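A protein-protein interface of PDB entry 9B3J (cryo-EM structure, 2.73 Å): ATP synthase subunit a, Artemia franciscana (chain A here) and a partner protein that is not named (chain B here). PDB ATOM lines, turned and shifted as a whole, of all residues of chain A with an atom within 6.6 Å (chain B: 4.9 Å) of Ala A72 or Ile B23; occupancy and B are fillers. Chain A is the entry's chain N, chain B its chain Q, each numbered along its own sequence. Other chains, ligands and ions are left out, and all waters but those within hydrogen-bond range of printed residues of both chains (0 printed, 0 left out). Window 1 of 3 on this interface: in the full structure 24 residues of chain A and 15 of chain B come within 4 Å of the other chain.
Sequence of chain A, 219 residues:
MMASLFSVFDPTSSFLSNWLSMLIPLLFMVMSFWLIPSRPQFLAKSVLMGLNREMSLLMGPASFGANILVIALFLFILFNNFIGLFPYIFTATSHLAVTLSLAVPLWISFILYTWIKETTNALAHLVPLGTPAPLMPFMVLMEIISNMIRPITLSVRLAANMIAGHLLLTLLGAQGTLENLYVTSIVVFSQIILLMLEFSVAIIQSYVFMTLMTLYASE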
ATOM      1  N   MET A  22     -30.213  -1.957 -25.971  1.00  0.00           N
ATOM      2  CA  MET A  22     -29.667  -1.967 -24.619  1.00  0.00           C
ATOM      3  C   MET A  22     -28.512  -0.996 -24.427  1.00  0.00           C
ATOM      4  O   MET A  22     -28.157  -0.699 -23.282  1.00  0.00           O
ATOM      5  CB  MET A  22     -29.205  -3.374 -24.258  1.00  0.00           C
ATOM      6  CG  MET A  22     -30.313  -4.388 -24.297  1.00  0.00           C
ATOM      7  SD  MET A  22     -29.688  -6.050 -24.073  1.00  0.00           S
ATOM      8  CE  MET A  22     -31.224  -6.945 -24.083  1.00  0.00           C
ATOM      9  N   PRO A  25     -29.390   3.200 -22.727  1.00  0.00           N
ATOM     10  CA  PRO A  25     -29.107   3.844 -21.430  1.00  0.00           C
ATOM     11  C   PRO A  25     -27.706   4.407 -21.281  1.00  0.00           C
ATOM     12  O   PRO A  25     -27.492   5.243 -20.401  1.00  0.00           O
ATOM     13  CB  PRO A  25     -29.347   2.718 -20.424  1.00  0.00           C
ATOM     14  CG  PRO A  25     -30.358   1.912 -21.040  1.00  0.00           C
ATOM     15  CD  PRO A  25     -30.037   1.893 -22.494  1.00  0.00           C
ATOM     16  N   LEU A  26     -26.742   3.978 -22.091  1.00  0.00           N
ATOM     17  CA  LEU A  26     -25.435   4.620 -22.045  1.00  0.00           C
ATOM     18  C   LEU A  26     -25.481   6.011 -22.658  1.00  0.00           C
ATOM     19  O   LEU A  26     -24.667   6.871 -22.307  1.00  0.00           O
ATOM     20  CB  LEU A  26     -24.394   3.761 -22.756  1.00  0.00           C
ATOM     21  CG  LEU A  26     -24.184   2.345 -22.226  1.00  0.00           C
ATOM     22  CD1 LEU A  26     -22.976   1.725 -22.888  1.00  0.00           C
ATOM     23  CD2 LEU A  26     -24.030   2.343 -20.724  1.00  0.00           C
ATOM     24  N   MET A  29     -27.471   8.519 -19.912  1.00  0.00           N
ATOM     25  CA  MET A  29     -26.927   8.650 -18.569  1.00  0.00           C
ATOM     26  C   MET A  29     -26.059   9.895 -18.514  1.00  0.00           C
ATOM     27  O   MET A  29     -25.232  10.123 -19.402  1.00  0.00           O
ATOM     28  CB  MET A  29     -26.115   7.418 -18.178  1.00  0.00           C
ATOM     29  CG  MET A  29     -25.548   7.469 -16.770  1.00  0.00           C
ATOM     30  SD  MET A  29     -26.811   7.541 -15.488  1.00  0.00           S
ATOM     31  CE  MET A  29     -27.764   6.087 -15.892  1.00  0.00           C
ATOM     32  N   ASN A  67     -27.439  -0.639  -1.921  1.00  0.00           N
ATOM     33  CA  ASN A  67     -27.661   0.763  -2.251  1.00  0.00           C
ATOM     34  C   ASN A  67     -27.624   0.987  -3.754  1.00  0.00           C
ATOM     35  O   ASN A  67     -28.482   1.681  -4.306  1.00  0.00           O
ATOM     36  CB  ASN A  67     -26.617   1.636  -1.564  1.00  0.00           C
ATOM     37  CG  ASN A  67     -26.753   1.629  -0.066  1.00  0.00           C
ATOM     38  OD1 ASN A  67     -26.119   0.832   0.624  1.00  0.00           O
ATOM     39  ND2 ASN A  67     -27.587   2.520   0.454  1.00  0.00           N
ATOM     40  N   ILE A  68     -26.652   0.389  -4.435  1.00  0.00           N
ATOM     41  CA  ILE A  68     -26.433   0.653  -5.850  1.00  0.00           C
ATOM     42  C   ILE A  68     -26.936  -0.479  -6.735  1.00  0.00           C
ATOM     43  O   ILE A  68     -27.254  -0.237  -7.909  1.00  0.00           O
ATOM     44  CB  ILE A  68     -24.935   0.929  -6.099  1.00  0.00           C
ATOM     45  CG1 ILE A  68     -24.688   1.584  -7.448  1.00  0.00           C
ATOM     46  CG2 ILE A  68     -24.110  -0.333  -5.983  1.00  0.00           C
ATOM     47  CD1 ILE A  68     -23.264   1.984  -7.619  1.00  0.00           C
ATOM     48  N   LEU A  69     -27.067  -1.691  -6.200  1.00  0.00           N
ATOM     49  CA  LEU A  69     -27.439  -2.846  -7.004  1.00  0.00           C
ATOM     50  C   LEU A  69     -28.890  -2.796  -7.451  1.00  0.00           C
ATOM     51  O   LEU A  69     -29.245  -3.442  -8.439  1.00  0.00           O
ATOM     52  CB  LEU A  69     -27.187  -4.121  -6.206  1.00  0.00           C
ATOM     53  CG  LEU A  69     -27.029  -5.420  -6.978  1.00  0.00           C
ATOM     54  CD1 LEU A  69     -25.606  -5.544  -7.458  1.00  0.00           C
ATOM     55  CD2 LEU A  69     -27.421  -6.596  -6.103  1.00  0.00           C
ATOM     56  N   VAL A  70     -29.731  -2.049  -6.745  1.00  0.00           N
ATOM     57  CA  VAL A  70     -31.141  -1.956  -7.083  1.00  0.00           C
ATOM     58  C   VAL A  70     -31.388  -0.644  -7.806  1.00  0.00           C
ATOM     59  O   VAL A  70     -32.349  -0.514  -8.569  1.00  0.00           O
ATOM     60  CB  VAL A  70     -32.023  -2.065  -5.834  1.00  0.00           C
ATOM     61  CG1 VAL A  70     -33.367  -2.590  -6.211  1.00  0.00           C
ATOM     62  CG2 VAL A  70     -31.388  -2.980  -4.830  1.00  0.00           C
ATOM     63  N   ILE A  71     -30.530   0.345  -7.558  1.00  0.00           N
ATOM     64  CA  ILE A  71     -30.649   1.609  -8.276  1.00  0.00           C
ATOM     65  C   ILE A  71     -30.262   1.427  -9.737  1.00  0.00           C
ATOM     66  O   ILE A  71     -30.938   1.939 -10.639  1.00  0.00           O
ATOM     67  CB  ILE A  71     -29.817   2.696  -7.577  1.00  0.00           C
ATOM     68  CG1 ILE A  71     -30.610   3.247  -6.395  1.00  0.00           C
ATOM     69  CG2 ILE A  71     -29.439   3.810  -8.531  1.00  0.00           C
ATOM     70  CD1 ILE A  71     -29.944   4.382  -5.680  1.00  0.00           C
ATOM     71  N   ALA A  72     -29.202   0.665  -9.997  1.00  0.00           N
ATOM     72  CA  ALA A  72     -28.813   0.390 -11.374  1.00  0.00           C
ATOM     73  C   ALA A  72     -29.876  -0.424 -12.099  1.00  0.00           C
ATOM     74  O   ALA A  72     -30.125  -0.211 -13.290  1.00  0.00           O
ATOM     75  CB  ALA A  72     -27.475  -0.336 -11.407  1.00  0.00           C
ATOM     76  N   LEU A  73     -30.525  -1.347 -11.394  1.00  0.00           N
ATOM     77  CA  LEU A  73     -31.618  -2.102 -11.995  1.00  0.00           C
ATOM     78  C   LEU A  73     -32.826  -1.214 -12.263  1.00  0.00           C
ATOM     79  O   LEU A  73     -33.517  -1.385 -13.277  1.00  0.00           O
ATOM     80  CB  LEU A  73     -31.999  -3.271 -11.093  1.00  0.00           C
ATOM     81  CG  LEU A  73     -33.146  -4.152 -11.563  1.00  0.00           C
ATOM     82  CD1 LEU A  73     -32.810  -4.755 -12.901  1.00  0.00           C
ATOM     83  CD2 LEU A  73     -33.390  -5.227 -10.548  1.00  0.00           C
ATOM     84  N   PHE A  74     -33.091  -0.254 -11.374  1.00  0.00           N
ATOM     85  CA  PHE A  74     -34.188   0.677 -11.608  1.00  0.00           C
ATOM     86  C   PHE A  74     -33.934   1.531 -12.838  1.00  0.00           C
ATOM     87  O   PHE A  74     -34.834   1.717 -13.659  1.00  0.00           O
ATOM     88  CB  PHE A  74     -34.403   1.565 -10.388  1.00  0.00           C
ATOM     89  CG  PHE A  74     -35.404   2.672 -10.604  1.00  0.00           C
ATOM     90  CD1 PHE A  74     -36.763   2.417 -10.567  1.00  0.00           C
ATOM     91  CD2 PHE A  74     -34.984   3.973 -10.820  1.00  0.00           C
ATOM     92  CE1 PHE A  74     -37.675   3.433 -10.752  1.00  0.00           C
ATOM     93  CE2 PHE A  74     -35.897   4.986 -11.013  1.00  0.00           C
ATOM     94  CZ  PHE A  74     -37.238   4.717 -10.971  1.00  0.00           C
ATOM     95  N   LEU A  75     -32.717   2.055 -12.989  1.00  0.00           N
ATOM     96  CA  LEU A  75     -32.426   2.889 -14.150  1.00  0.00           C
ATOM     97  C   LEU A  75     -32.405   2.083 -15.439  1.00  0.00           C
ATOM     98  O   LEU A  75     -32.821   2.589 -16.488  1.00  0.00           O
ATOM     99  CB  LEU A  75     -31.100   3.612 -13.965  1.00  0.00           C
ATOM    100  CG  LEU A  75     -31.070   4.585 -12.798  1.00  0.00           C
ATOM    101  CD1 LEU A  75     -29.831   5.425 -12.896  1.00  0.00           C
ATOM    102  CD2 LEU A  75     -32.305   5.456 -12.793  1.00  0.00           C
ATOM    103  N   PHE A  76     -31.941   0.836 -15.383  1.00  0.00           N
ATOM    104  CA  PHE A  76     -31.957  -0.016 -16.565  1.00  0.00           C
ATOM    105  C   PHE A  76     -33.384  -0.280 -17.032  1.00  0.00           C
ATOM    106  O   PHE A  76     -33.711  -0.113 -18.222  1.00  0.00           O
ATOM    107  CB  PHE A  76     -31.233  -1.321 -16.245  1.00  0.00           C
ATOM    108  CG  PHE A  76     -31.029  -2.211 -17.426  1.00  0.00           C
ATOM    109  CD1 PHE A  76     -29.972  -2.005 -18.286  1.00  0.00           C
ATOM    110  CD2 PHE A  76     -31.881  -3.264 -17.665  1.00  0.00           C
ATOM    111  CE1 PHE A  76     -29.781  -2.819 -19.369  1.00  0.00           C
ATOM    112  CE2 PHE A  76     -31.694  -4.086 -18.744  1.00  0.00           C
ATOM    113  CZ  PHE A  76     -30.643  -3.862 -19.597  1.00  0.00           C
ATOM    114  N   ILE A  77     -34.260  -0.644 -16.095  1.00  0.00           N
ATOM    115  CA  ILE A  77     -35.646  -0.924 -16.447  1.00  0.00           C
ATOM    116  C   ILE A  77     -36.365   0.346 -16.873  1.00  0.00           C
ATOM    117  O   ILE A  77     -37.146   0.339 -17.833  1.00  0.00           O
ATOM    118  CB  ILE A  77     -36.349  -1.611 -15.266  1.00  0.00           C
ATOM    119  CG1 ILE A  77     -35.763  -2.997 -15.056  1.00  0.00           C
ATOM    120  CG2 ILE A  77     -37.825  -1.718 -15.500  1.00  0.00           C
ATOM    121  CD1 ILE A  77     -36.311  -3.683 -13.862  1.00  0.00           C
ATOM    122  N   PHE A  79     -35.120   3.190 -18.238  1.00  0.00           N
ATOM    123  CA  PHE A  79     -34.723   3.706 -19.541  1.00  0.00           C
ATOM    124  C   PHE A  79     -35.230   2.826 -20.671  1.00  0.00           C
ATOM    125  O   PHE A  79     -35.625   3.341 -21.724  1.00  0.00           O
ATOM    126  CB  PHE A  79     -33.210   3.842 -19.627  1.00  0.00           C
ATOM    127  CG  PHE A  79     -32.664   4.992 -18.850  1.00  0.00           C
ATOM    128  CD1 PHE A  79     -33.490   6.012 -18.421  1.00  0.00           C
ATOM    129  CD2 PHE A  79     -31.318   5.053 -18.548  1.00  0.00           C
ATOM    130  CE1 PHE A  79     -32.984   7.068 -17.704  1.00  0.00           C
ATOM    131  CE2 PHE A  79     -30.807   6.105 -17.833  1.00  0.00           C
ATOM    132  CZ  PHE A  79     -31.641   7.116 -17.409  1.00  0.00           C
ATOM    133  N   LEU B  19     -24.434  -4.563 -19.399  1.00  0.00           N
ATOM    134  CA  LEU B  19     -25.028  -3.233 -19.379  1.00  0.00           C
ATOM    135  C   LEU B  19     -25.506  -2.856 -17.986  1.00  0.00           C
ATOM    136  O   LEU B  19     -25.420  -1.690 -17.597  1.00  0.00           O
ATOM    137  CB  LEU B  19     -26.179  -3.160 -20.376  1.00  0.00           C
ATOM    138  CG  LEU B  19     -25.821  -2.506 -21.703  1.00  0.00           C
ATOM    139  CD1 LEU B  19     -25.292  -1.123 -21.431  1.00  0.00           C
ATOM    140  CD2 LEU B  19     -24.796  -3.317 -22.463  1.00  0.00           C
ATOM    141  N   LEU B  20     -26.025  -3.819 -17.224  1.00  0.00           N
ATOM    142  CA  LEU B  20     -26.434  -3.531 -15.856  1.00  0.00           C
ATOM    143  C   LEU B  20     -25.235  -3.204 -14.982  1.00  0.00           C
ATOM    144  O   LEU B  20     -25.312  -2.330 -14.112  1.00  0.00           O
ATOM    145  CB  LEU B  20     -27.206  -4.708 -15.281  1.00  0.00           C
ATOM    146  CG  LEU B  20     -27.768  -4.513 -13.883  1.00  0.00           C
ATOM    147  CD1 LEU B  20     -28.625  -3.285 -13.853  1.00  0.00           C
ATOM    148  CD2 LEU B  20     -28.577  -5.721 -13.505  1.00  0.00           C
ATOM    149  N   TRP B  21     -24.108  -3.875 -15.213  1.00  0.00           N
ATOM    150  CA  TRP B  21     -22.884  -3.491 -14.522  1.00  0.00           C
ATOM    151  C   TRP B  21     -22.355  -2.149 -15.011  1.00  0.00           C
ATOM    152  O   TRP B  21     -21.768  -1.392 -14.230  1.00  0.00           O
ATOM    153  CB  TRP B  21     -21.815  -4.561 -14.694  1.00  0.00           C
ATOM    154  CG  TRP B  21     -20.744  -4.451 -13.688  1.00  0.00           C
ATOM    155  CD1 TRP B  21     -20.796  -4.879 -12.404  1.00  0.00           C
ATOM    156  CD2 TRP B  21     -19.452  -3.873 -13.870  1.00  0.00           C
ATOM    157  NE1 TRP B  21     -19.615  -4.606 -11.768  1.00  0.00           N
ATOM    158  CE2 TRP B  21     -18.771  -3.987 -12.650  1.00  0.00           C
ATOM    159  CE3 TRP B  21     -18.801  -3.274 -14.945  1.00  0.00           C
ATOM    160  CZ2 TRP B  21     -17.477  -3.522 -12.473  1.00  0.00           C
ATOM    161  CZ3 TRP B  21     -17.516  -2.814 -14.768  1.00  0.00           C
ATOM    162  CH2 TRP B  21     -16.868  -2.941 -13.542  1.00  0.00           C
ATOM    163  N   ALA B  22     -22.547  -1.833 -16.290  1.00  0.00           N
ATOM    164  CA  ALA B  22     -22.127  -0.528 -16.778  1.00  0.00           C
ATOM    165  C   ALA B  22     -22.981   0.584 -16.186  1.00  0.00           C
ATOM    166  O   ALA B  22     -22.475   1.668 -15.887  1.00  0.00           O
ATOM    167  CB  ALA B  22     -22.173  -0.494 -18.299  1.00  0.00           C
ATOM    168  N   ILE B  23     -24.274   0.337 -15.991  1.00  0.00           N
ATOM    169  CA  ILE B  23     -25.124   1.328 -15.338  1.00  0.00           C
ATOM    170  C   ILE B  23     -24.739   1.468 -13.872  1.00  0.00           C
ATOM    171  O   ILE B  23     -24.753   2.572 -13.309  1.00  0.00           O
ATOM    172  CB  ILE B  23     -26.605   0.956 -15.520  1.00  0.00           C
ATOM    173  CG1 ILE B  23     -27.010   1.207 -16.966  1.00  0.00           C
ATOM    174  CG2 ILE B  23     -27.499   1.743 -14.589  1.00  0.00           C
ATOM    175  CD1 ILE B  23     -28.469   1.047 -17.225  1.00  0.00           C
ATOM    176  N   MET B  24     -24.350   0.356 -13.245  1.00  0.00           N
ATOM    177  CA  MET B  24     -23.884   0.392 -11.863  1.00  0.00           C
ATOM    178  C   MET B  24     -22.642   1.259 -11.718  1.00  0.00           C
ATOM    179  O   MET B  24     -22.565   2.103 -10.822  1.00  0.00           O
ATOM    180  CB  MET B  24     -23.604  -1.029 -11.389  1.00  0.00           C
ATOM    181  CG  MET B  24     -23.456  -1.176  -9.902  1.00  0.00           C
ATOM    182  SD  MET B  24     -23.106  -2.879  -9.470  1.00  0.00           S
ATOM    183  CE  MET B  24     -24.354  -3.700 -10.444  1.00  0.00           C
ATOM    184  N   THR B  25     -21.673   1.095 -12.608  1.00  0.00           N
ATOM    185  CA  THR B  25     -20.495   1.941 -12.502  1.00  0.00           C
ATOM    186  C   THR B  25     -20.703   3.342 -13.057  1.00  0.00           C
ATOM    187  O   THR B  25     -19.803   4.172 -12.920  1.00  0.00           O
ATOM    188  CB  THR B  25     -19.302   1.321 -13.204  1.00  0.00           C
ATOM    189  OG1 THR B  25     -18.230   2.260 -13.176  1.00  0.00           O
ATOM    190  CG2 THR B  25     -19.610   1.051 -14.621  1.00  0.00           C
ATOM    191  N   MET B  26     -21.826   3.619 -13.719  1.00  0.00           N
ATOM    192  CA  MET B  26     -22.137   5.008 -14.040  1.00  0.00           C
ATOM    193  C   MET B  26     -22.755   5.727 -12.848  1.00  0.00           C
ATOM    194  O   MET B  26     -22.464   6.902 -12.610  1.00  0.00           O
ATOM    195  CB  MET B  26     -23.080   5.091 -15.242  1.00  0.00           C
ATOM    196  CG  MET B  26     -22.461   4.746 -16.593  1.00  0.00           C
ATOM    197  SD  MET B  26     -21.139   5.839 -17.133  1.00  0.00           S
ATOM    198  CE  MET B  26     -22.068   7.116 -17.971  1.00  0.00           C
ATOM    199  N   VAL B  27     -23.619   5.036 -12.099  1.00  0.00           N
ATOM    200  CA  VAL B  27     -24.220   5.619 -10.902  1.00  0.00           C
ATOM    201  C   VAL B  27     -23.185   5.788  -9.800  1.00  0.00           C
ATOM    202  O   VAL B  27     -23.253   6.743  -9.017  1.00  0.00           O
ATOM    203  CB  VAL B  27     -25.411   4.755 -10.449  1.00  0.00           C
ATOM    204  CG1 VAL B  27     -26.035   5.286  -9.191  1.00  0.00           C
ATOM    205  CG2 VAL B  27     -26.451   4.733 -11.521  1.00  0.00           C
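Asn A67 touches none of the printed residues of chain B.
Val A70 touches none of the printed residues of chain B.
Of the printed residues of chain B, Ile A71 touches Val B27 (3.8 Å).
Of chain B, only Leu B20, Ile B23 and Met B24 come within 4 Å of Ala A72.
Of the printed residues of chain B, Leu A73 touches Leu B20 (3.7 Å).
Ile B23 touches just these residues of chain A: Pro A25, Ala A72 and Phe A76.
The nearest residue of chain A that does not touch Ile B23 is Leu A75 (4.1 Å).
Among the printed residues, merely in contact across the chains: Ile A68 with Met B24, Met A22 with Leu B19, Ala A72 with Leu B20, Ala A72 with Ile B23, Phe A76 with Ile B23, Leu A73 with Leu B20, Ala A72 with Met B24, Met A29 with Met B26, Leu A75 with Val B27, Pro A25 with Ile B23, Leu A69 with Met B24, Leu A26 with Leu B19, Phe A76 with Leu B19 and Ile A71 with Val B27.
Printed residues of chain A that touch a printed residue of chain B: Met A22, Pro A25, Leu A26, Met A29, Ile A68, Leu A69, Ile A71, Ala A72, Leu A73, Leu A75 and Phe A76.
Printed residues of chain B that touch a printed residue of chain A: Leu B19, Leu B20, Ile B23, Met B24, Met B26 and Val B27.
Hydrophobic or aromatic side chains of chain B that line the printed part of chain A: Leu B19, Leu B20, Ile B23, Met B24, Met B26 and Val B27.
Among the printed residues, no Asp or Glu carboxylate lies within 4 Å of a Lys or Arg side-chain nitrogen of the other chain.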
